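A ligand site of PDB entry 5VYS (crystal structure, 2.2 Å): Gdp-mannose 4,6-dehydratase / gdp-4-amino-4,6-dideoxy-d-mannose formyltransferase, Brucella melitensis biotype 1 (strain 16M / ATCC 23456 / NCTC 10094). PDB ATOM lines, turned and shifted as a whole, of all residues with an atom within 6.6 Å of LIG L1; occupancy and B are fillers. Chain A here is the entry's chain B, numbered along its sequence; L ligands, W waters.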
ATOM      1  N   TYR A  89      -8.535  -0.155 -17.524  1.00  0.00           N
ATOM      2  CA  TYR A  89      -8.089  -1.090 -18.545  1.00  0.00           C
ATOM      3  C   TYR A  89      -8.920  -0.822 -19.788  1.00  0.00           C
ATOM      4  O   TYR A  89     -10.052  -0.461 -19.702  1.00  0.00           O
ATOM      5  CB  TYR A  89      -8.238  -2.533 -18.026  1.00  0.00           C
ATOM      6  CG  TYR A  89      -7.570  -3.562 -18.880  1.00  0.00           C
ATOM      7  CD1 TYR A  89      -8.321  -4.412 -19.677  1.00  0.00           C
ATOM      8  CD2 TYR A  89      -6.188  -3.693 -18.912  1.00  0.00           C
ATOM      9  CE1 TYR A  89      -7.706  -5.408 -20.461  1.00  0.00           C
ATOM     10  CE2 TYR A  89      -5.582  -4.649 -19.713  1.00  0.00           C
ATOM     11  CZ  TYR A  89      -6.346  -5.496 -20.496  1.00  0.00           C
ATOM     12  OH  TYR A  89      -5.774  -6.447 -21.318  1.00  0.00           O
ATOM     13  N   ARG A  90      -8.378  -1.032 -20.970  1.00  0.00           N
ATOM     14  CA  ARG A  90      -8.932  -0.451 -22.207  1.00  0.00           C
ATOM     15  C   ARG A  90      -9.397  -1.499 -23.206  1.00  0.00           C
ATOM     16  O   ARG A  90      -9.606  -1.190 -24.386  1.00  0.00           O
ATOM     17  CB  ARG A  90      -7.944   0.490 -22.885  1.00  0.00           C
ATOM     18  CG  ARG A  90      -7.497   1.654 -22.027  1.00  0.00           C
ATOM     19  CD  ARG A  90      -6.386   2.412 -22.730  1.00  0.00           C
ATOM     20  NE  ARG A  90      -6.846   3.093 -23.939  1.00  0.00           N
ATOM     21  CZ  ARG A  90      -7.428   4.305 -23.962  1.00  0.00           C
ATOM     22  NH1 ARG A  90      -7.662   5.031 -22.844  1.00  0.00           N
ATOM     23  NH2 ARG A  90      -7.794   4.801 -25.138  1.00  0.00           N
ATOM     24  N   SER A  91      -9.605  -2.723 -22.722  1.00  0.00           N
ATOM     25  CA  SER A  91     -10.014  -3.822 -23.583  1.00  0.00           C
ATOM     26  C   SER A  91     -11.098  -4.594 -22.866  1.00  0.00           C
ATOM     27  O   SER A  91     -11.178  -4.590 -21.597  1.00  0.00           O
ATOM     28  CB  SER A  91      -8.851  -4.737 -23.860  1.00  0.00           C
ATOM     29  OG  SER A  91      -7.815  -4.044 -24.509  1.00  0.00           O
ATOM     30  N   LEU A  92     -11.926  -5.250 -23.667  1.00  0.00           N
ATOM     31  CA  LEU A  92     -12.892  -6.236 -23.156  1.00  0.00           C
ATOM     32  C   LEU A  92     -12.119  -7.408 -22.557  1.00  0.00           C
ATOM     33  O   LEU A  92     -11.212  -7.941 -23.168  1.00  0.00           O
ATOM     34  CB  LEU A  92     -13.864  -6.717 -24.251  1.00  0.00           C
ATOM     35  CG  LEU A  92     -14.949  -7.686 -23.762  1.00  0.00           C
ATOM     36  CD1 LEU A  92     -15.970  -6.910 -22.946  1.00  0.00           C
ATOM     37  CD2 LEU A  92     -15.649  -8.393 -24.894  1.00  0.00           C
ATOM     38  N   ASN A 107     -14.910  -3.043 -11.865  1.00  0.00           N
ATOM     39  CA  ASN A 107     -14.427  -2.086 -12.844  1.00  0.00           C
ATOM     40  C   ASN A 107     -14.955  -0.705 -12.482  1.00  0.00           C
ATOM     41  O   ASN A 107     -16.046  -0.586 -11.963  1.00  0.00           O
ATOM     42  CB  ASN A 107     -14.874  -2.446 -14.284  1.00  0.00           C
ATOM     43  CG  ASN A 107     -14.507  -1.362 -15.292  1.00  0.00           C
ATOM     44  OD1 ASN A 107     -15.376  -0.635 -15.806  1.00  0.00           O
ATOM     45  ND2 ASN A 107     -13.237  -1.195 -15.526  1.00  0.00           N
ATOM     46  N   HIS A 109     -16.302   2.798 -13.821  1.00  0.00           N
ATOM     47  CA  HIS A 109     -16.875   3.394 -15.023  1.00  0.00           C
ATOM     48  C   HIS A 109     -17.303   4.818 -14.700  1.00  0.00           C
ATOM     49  O   HIS A 109     -17.967   5.026 -13.680  1.00  0.00           O
ATOM     50  CB  HIS A 109     -18.090   2.596 -15.479  1.00  0.00           C
ATOM     51  CG  HIS A 109     -18.623   3.078 -16.788  1.00  0.00           C
ATOM     52  ND1 HIS A 109     -18.034   2.759 -17.985  1.00  0.00           N
ATOM     53  CD2 HIS A 109     -19.649   3.905 -17.081  1.00  0.00           C
ATOM     54  CE1 HIS A 109     -18.685   3.361 -18.967  1.00  0.00           C
ATOM     55  NE2 HIS A 109     -19.673   4.063 -18.444  1.00  0.00           N
ATOM     56  N   PRO A 110     -16.997   5.789 -15.572  1.00  0.00           N
ATOM     57  CA  PRO A 110     -17.254   7.209 -15.222  1.00  0.00           C
ATOM     58  C   PRO A 110     -18.678   7.719 -15.540  1.00  0.00           C
ATOM     59  O   PRO A 110     -18.838   8.778 -16.152  1.00  0.00           O
ATOM     60  CB  PRO A 110     -16.205   7.939 -16.050  1.00  0.00           C
ATOM     61  CG  PRO A 110     -16.172   7.112 -17.301  1.00  0.00           C
ATOM     62  CD  PRO A 110     -16.246   5.684 -16.840  1.00  0.00           C
ATOM     63  N   ARG A 117     -23.775   4.163 -20.711  1.00  0.00           N
ATOM     64  CA  ARG A 117     -22.994   3.032 -21.149  1.00  0.00           C
ATOM     65  C   ARG A 117     -22.224   3.483 -22.389  1.00  0.00           C
ATOM     66  O   ARG A 117     -22.585   4.489 -23.031  1.00  0.00           O
ATOM     67  CB  ARG A 117     -23.871   1.830 -21.426  1.00  0.00           C
ATOM     68  CG  ARG A 117     -24.337   1.217 -20.107  1.00  0.00           C
ATOM     69  CD  ARG A 117     -25.157  -0.040 -20.303  1.00  0.00           C
ATOM     70  NE  ARG A 117     -25.590  -0.569 -19.012  1.00  0.00           N
ATOM     71  CZ  ARG A 117     -26.506  -1.515 -18.858  1.00  0.00           C
ATOM     72  NH1 ARG A 117     -26.805  -1.917 -17.647  1.00  0.00           N
ATOM     73  NH2 ARG A 117     -27.146  -2.064 -19.909  1.00  0.00           N
ATOM     74  N   GLY A 118     -21.149   2.784 -22.686  1.00  0.00           N
ATOM     75  CA  GLY A 118     -20.273   3.177 -23.781  1.00  0.00           C
ATOM     76  C   GLY A 118     -19.018   3.907 -23.343  1.00  0.00           C
ATOM     77  O   GLY A 118     -18.565   3.791 -22.191  1.00  0.00           O
ATOM     78  N   THR A 119     -18.467   4.653 -24.295  1.00  0.00           N
ATOM     79  CA  THR A 119     -17.256   5.380 -24.153  1.00  0.00           C
ATOM     80  C   THR A 119     -17.589   6.857 -24.202  1.00  0.00           C
ATOM     81  O   THR A 119     -18.710   7.198 -24.541  1.00  0.00           O
ATOM     82  CB  THR A 119     -16.361   5.094 -25.368  1.00  0.00           C
ATOM     83  OG1 THR A 119     -17.108   5.342 -26.568  1.00  0.00           O
ATOM     84  CG2 THR A 119     -15.866   3.642 -25.336  1.00  0.00           C
ATOM     85  N   PHE A 144     -19.326  -5.075 -21.603  1.00  0.00           N
ATOM     86  CA  PHE A 144     -19.021  -3.816 -21.006  1.00  0.00           C
ATOM     87  C   PHE A 144     -20.263  -3.227 -20.311  1.00  0.00           C
ATOM     88  O   PHE A 144     -21.405  -3.262 -20.859  1.00  0.00           O
ATOM     89  CB  PHE A 144     -18.647  -2.819 -22.101  1.00  0.00           C
ATOM     90  CG  PHE A 144     -17.293  -3.003 -22.703  1.00  0.00           C
ATOM     91  CD1 PHE A 144     -16.173  -2.780 -21.961  1.00  0.00           C
ATOM     92  CD2 PHE A 144     -17.156  -3.285 -24.053  1.00  0.00           C
ATOM     93  CE1 PHE A 144     -14.910  -2.898 -22.524  1.00  0.00           C
ATOM     94  CE2 PHE A 144     -15.898  -3.391 -24.624  1.00  0.00           C
ATOM     95  CZ  PHE A 144     -14.777  -3.208 -23.859  1.00  0.00           C
ATOM     96  N   ASP A 145     -20.021  -2.660 -19.130  1.00  0.00           N
ATOM     97  CA  ASP A 145     -20.879  -1.667 -18.499  1.00  0.00           C
ATOM     98  C   ASP A 145     -22.170  -2.202 -17.894  1.00  0.00           C
ATOM     99  O   ASP A 145     -23.042  -1.397 -17.535  1.00  0.00           O
ATOM    100  CB  ASP A 145     -21.263  -0.527 -19.476  1.00  0.00           C
ATOM    101  CG  ASP A 145     -20.111  -0.016 -20.298  1.00  0.00           C
ATOM    102  OD1 ASP A 145     -18.979   0.099 -19.790  1.00  0.00           O
ATOM    103  OD2 ASP A 145     -20.352   0.318 -21.486  1.00  0.00           O
ATOM    104  N   TYR A 200     -26.905   4.903 -24.261  1.00  0.00           N
ATOM    105  CA  TYR A 200     -25.752   4.387 -24.989  1.00  0.00           C
ATOM    106  C   TYR A 200     -25.135   5.426 -25.953  1.00  0.00           C
ATOM    107  O   TYR A 200     -25.856   6.183 -26.598  1.00  0.00           O
ATOM    108  CB  TYR A 200     -26.184   3.135 -25.755  1.00  0.00           C
ATOM    109  CG  TYR A 200     -26.681   1.990 -24.891  1.00  0.00           C
ATOM    110  CD1 TYR A 200     -25.827   0.929 -24.562  1.00  0.00           C
ATOM    111  CD2 TYR A 200     -27.993   1.926 -24.423  1.00  0.00           C
ATOM    112  CE1 TYR A 200     -26.271  -0.149 -23.787  1.00  0.00           C
ATOM    113  CE2 TYR A 200     -28.434   0.868 -23.650  1.00  0.00           C
ATOM    114  CZ  TYR A 200     -27.556  -0.179 -23.357  1.00  0.00           C
ATOM    115  OH  TYR A 200     -27.946  -1.235 -22.591  1.00  0.00           O
ATOM    116  N   TYR A 201     -23.800   5.461 -26.038  1.00  0.00           N
ATOM    117  CA  TYR A 201     -23.095   6.466 -26.852  1.00  0.00           C
ATOM    118  C   TYR A 201     -21.867   5.880 -27.548  1.00  0.00           C
ATOM    119  O   TYR A 201     -20.942   5.386 -26.900  1.00  0.00           O
ATOM    120  CB  TYR A 201     -22.725   7.732 -26.008  1.00  0.00           C
ATOM    121  CG  TYR A 201     -23.950   8.430 -25.461  1.00  0.00           C
ATOM    122  CD1 TYR A 201     -24.681   9.354 -26.209  1.00  0.00           C
ATOM    123  CD2 TYR A 201     -24.429   8.110 -24.190  1.00  0.00           C
ATOM    124  CE1 TYR A 201     -25.843   9.949 -25.705  1.00  0.00           C
ATOM    125  CE2 TYR A 201     -25.572   8.692 -23.679  1.00  0.00           C
ATOM    126  CZ  TYR A 201     -26.275   9.611 -24.440  1.00  0.00           C
ATOM    127  OH  TYR A 201     -27.411  10.145 -23.869  1.00  0.00           O
ATOM    128  N   ARG A 203     -18.697   4.504 -30.066  1.00  0.00           N
ATOM    129  CA  ARG A 203     -17.246   4.452 -29.805  1.00  0.00           C
ATOM    130  C   ARG A 203     -16.535   5.787 -30.060  1.00  0.00           C
ATOM    131  O   ARG A 203     -15.735   6.217 -29.222  1.00  0.00           O
ATOM    132  CB  ARG A 203     -16.557   3.331 -30.632  1.00  0.00           C
ATOM    133  CG  ARG A 203     -15.167   2.929 -30.129  1.00  0.00           C
ATOM    134  CD  ARG A 203     -14.236   2.314 -31.182  1.00  0.00           C
ATOM    135  NE  ARG A 203     -14.273   0.848 -31.201  1.00  0.00           N
ATOM    136  CZ  ARG A 203     -13.309   0.034 -31.653  1.00  0.00           C
ATOM    137  NH1 ARG A 203     -13.488  -1.285 -31.617  1.00  0.00           N
ATOM    138  NH2 ARG A 203     -12.169   0.518 -32.140  1.00  0.00           N
HETATM  139  O1  LIG L   1     -11.151   2.970 -28.543  1.00  0.00           O
HETATM  140  C1  LIG L   1     -12.165   1.938 -28.539  1.00  0.00           C
HETATM  141  C2  LIG L   1     -12.114   1.017 -27.312  1.00  0.00           C
HETATM  142  O2  LIG L   1     -13.168   1.339 -26.388  1.00  0.00           O
HETATM  143  C3  LIG L   1     -12.255  -0.480 -27.597  1.00  0.00           C
HETATM  144  O3  LIG L   1     -10.994  -1.172 -27.656  1.00  0.00           O
HETATM  145  C4  LIG L   1     -12.991  -1.030 -26.401  1.00  0.00           C
HETATM  146  O4  LIG L   1     -12.056  -1.694 -25.551  1.00  0.00           O
HETATM  147  C5  LIG L   1     -13.631   0.176 -25.715  1.00  0.00           C
HETATM  148  N1  LIG L   1     -15.127   0.076 -25.773  1.00  0.00           N
HETATM  149  C6  LIG L   1     -15.887  -0.184 -26.863  1.00  0.00           C
HETATM  150  N2  LIG L   1     -17.209  -0.216 -26.552  1.00  0.00           N
HETATM  151  C7  LIG L   1     -17.312   0.057 -25.237  1.00  0.00           C
HETATM  152  C8  LIG L   1     -18.423   0.189 -24.258  1.00  0.00           C
HETATM  153  O5  LIG L   1     -19.613   0.024 -24.584  1.00  0.00           O
HETATM  154  N3  LIG L   1     -18.112   0.458 -22.974  1.00  0.00           N
HETATM  155  C9  LIG L   1     -16.846   0.648 -22.564  1.00  0.00           C
HETATM  156  N4  LIG L   1     -16.623   0.902 -21.250  1.00  0.00           N
HETATM  157  N5  LIG L   1     -15.766   0.551 -23.396  1.00  0.00           N
HETATM  158  C10 LIG L   1     -15.953   0.249 -24.722  1.00  0.00           C
HETATM  159  N1  LG2 L   2     -16.718  -6.477 -18.524  1.00  0.00           N
HETATM  160  C1  LG2 L   2     -15.618  -7.102 -19.011  1.00  0.00           C
HETATM  161  N2  LG2 L   2     -14.481  -6.401 -19.292  1.00  0.00           N
HETATM  162  C2  LG2 L   2     -14.345  -5.083 -19.129  1.00  0.00           C
HETATM  163  C3  LG2 L   2     -15.496  -4.318 -18.623  1.00  0.00           C
HETATM  164  C4  LG2 L   2     -16.722  -5.136 -18.334  1.00  0.00           C
HETATM  165  N3  LG2 L   2     -13.218  -4.443 -19.435  1.00  0.00           N
HETATM  166  C5  LG2 L   2     -13.078  -3.097 -19.289  1.00  0.00           C
HETATM  167  C6  LG2 L   2     -14.157  -2.192 -18.813  1.00  0.00           C
HETATM  168  N4  LG2 L   2     -15.381  -2.905 -18.459  1.00  0.00           N
HETATM  169  O1  LG2 L   2     -17.763  -4.593 -17.871  1.00  0.00           O
HETATM  170  N5  LG2 L   2     -15.700  -8.449 -19.186  1.00  0.00           N
HETATM  171  P1  LG3 L   3     -12.743   6.047 -23.150  1.00  0.00           P
HETATM  172  O1  LG3 L   3     -13.971   6.773 -22.655  1.00  0.00           O
HETATM  173  O2  LG3 L   3     -12.512   4.652 -22.552  1.00  0.00           O
HETATM  174  O3  LG3 L   3     -12.628   6.083 -24.662  1.00  0.00           O
HETATM  175  O4  LG3 L   3     -11.600   7.031 -22.493  1.00  0.00           O
HETATM  176  P2  LG3 L   3     -10.219   7.642 -23.124  1.00  0.00           P
HETATM  177  O5  LG3 L   3      -9.152   7.662 -22.036  1.00  0.00           O
HETATM  178  O6  LG3 L   3      -9.892   7.148 -24.499  1.00  0.00           O
HETATM  179  O7  LG3 L   3     -10.711   9.155 -23.295  1.00  0.00           O
HETATM  180  C1  LG3 L   3     -11.091   9.916 -22.143  1.00  0.00           C
HETATM  181  C2  LG3 L   3     -11.676  11.243 -22.591  1.00  0.00           C
HETATM  182  O8  LG3 L   3     -10.720  11.967 -23.397  1.00  0.00           O
HETATM  183  C3  LG3 L   3     -12.955  11.100 -23.408  1.00  0.00           C
HETATM  184  O9  LG3 L   3     -14.130  11.049 -22.580  1.00  0.00           O
HETATM  185  C4  LG3 L   3     -12.913  12.357 -24.232  1.00  0.00           C
HETATM  186  O10 LG3 L   3     -13.593  13.352 -23.468  1.00  0.00           O
HETATM  187  C5  LG3 L   3     -11.438  12.743 -24.369  1.00  0.00           C
HETATM  188  N1  LG3 L   3     -10.911  12.433 -25.714  1.00  0.00           N
HETATM  189  C6  LG3 L   3     -10.452  11.213 -26.093  1.00  0.00           C
HETATM  190  N2  LG3 L   3     -10.013  11.225 -27.380  1.00  0.00           N
HETATM  191  C7  LG3 L   3     -10.207  12.482 -27.827  1.00  0.00           C
HETATM  192  C8  LG3 L   3      -9.962  13.192 -29.115  1.00  0.00           C
HETATM  193  O11 LG3 L   3      -9.464  12.557 -30.078  1.00  0.00           O
HETATM  194  N3  LG3 L   3     -10.281  14.481 -29.209  1.00  0.00           N
HETATM  195  C9  LG3 L   3     -10.808  15.167 -28.157  1.00  0.00           C
HETATM  196  N4  LG3 L   3     -11.102  16.478 -28.316  1.00  0.00           N
HETATM  197  N5  LG3 L   3     -11.048  14.583 -26.949  1.00  0.00           N
HETATM  198  C10 LG3 L   3     -10.783  13.270 -26.718  1.00  0.00           C
HETATM  199  O   HOH W   1     -11.250   5.905 -26.973  1.00  0.00           O
HETATM  200  O   HOH W   2     -19.922  -2.872 -26.508  1.00  0.00           O
HETATM  201  O   HOH W   3      -9.466   3.671 -26.455  1.00  0.00           O
HETATM  202  O   HOH W   4     -11.693  -4.964 -26.507  1.00  0.00           O
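OD2 of Asp 145 is in hydrogen-bond range of N3 of LIG L1 (2.7 Å).
O of Arg 90 sits at hydrogen-bond distance from O4 of LIG L1, at 2.8 Å.
N3 of LIG L1 lies within hydrogen-bond range of O of Gly 118.
N of Asp 145 is in hydrogen-bond range of O1 of LG2 L2 (3.2 Å).
O of Ser 91 lies within hydrogen-bond range of N3 of LG2 L2, 3.0 Å away.
The side-chain amide oxygen of Asn 107 is in hydrogen-bond range of a nitrogen (N4) of LG2 L2 (3.5 Å).
NH1 of Arg 90 is in salt-bridge range of O5 of LG3 L3.
The side-chain carboxylate (OD2) of Asp 145 is in hydrogen-bond range of the backbone NH (N) of Gly 118 (2.9 Å).
The side-chain carboxylate of Asp 145 lies within hydrogen-bond range of a ring nitrogen (ND1) of His 109 (3.4 Å).
The guanidinium group (NE) of Arg 117 lies within hydrogen-bond range of the backbone carbonyl oxygen (O) of Asp 145 (3.1 Å).
The backbone carbonyl oxygen of Arg 203 lies within hydrogen-bond range of the side-chain hydroxyl of Thr 119 (3.1 Å).
CA of Ser 91 touches O4 of LIG L1, at 3.5 Å.
His 109 touches LIG L1 (CE1 to N4, 3.9 Å).
CG2 of Thr 119 touches C10 of LIG L1, at 3.4 Å.
CB of Phe 144 touches N3 of LIG L1 (3.4 Å).
Arg 203 touches LIG L1 (CD to C1, 3.4 Å).
Hydrophobic or aromatic side chains within 4 Å of LIG L1: His 109 and Phe 144.
Along chain A the residues within 4 Å of LIG L1 span positions 90 to 203.
The nearest printed residue that does not touch LIG L1 is Leu 92 (4.03 Å).
Water W3 lies within hydrogen-bond range of NH2 of Arg 90 (2.4 Å) and O1 of LIG L1 (2.8 Å).
Water W1 bridges O3 of LG3 L3 (2.7 Å) and O1 of LIG L1 (3.3 Å).
Water W4 bridges the backbone NH of Leu 92 (2.9 Å) and an oxygen (O4) of LIG L1 (3.4 Å).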
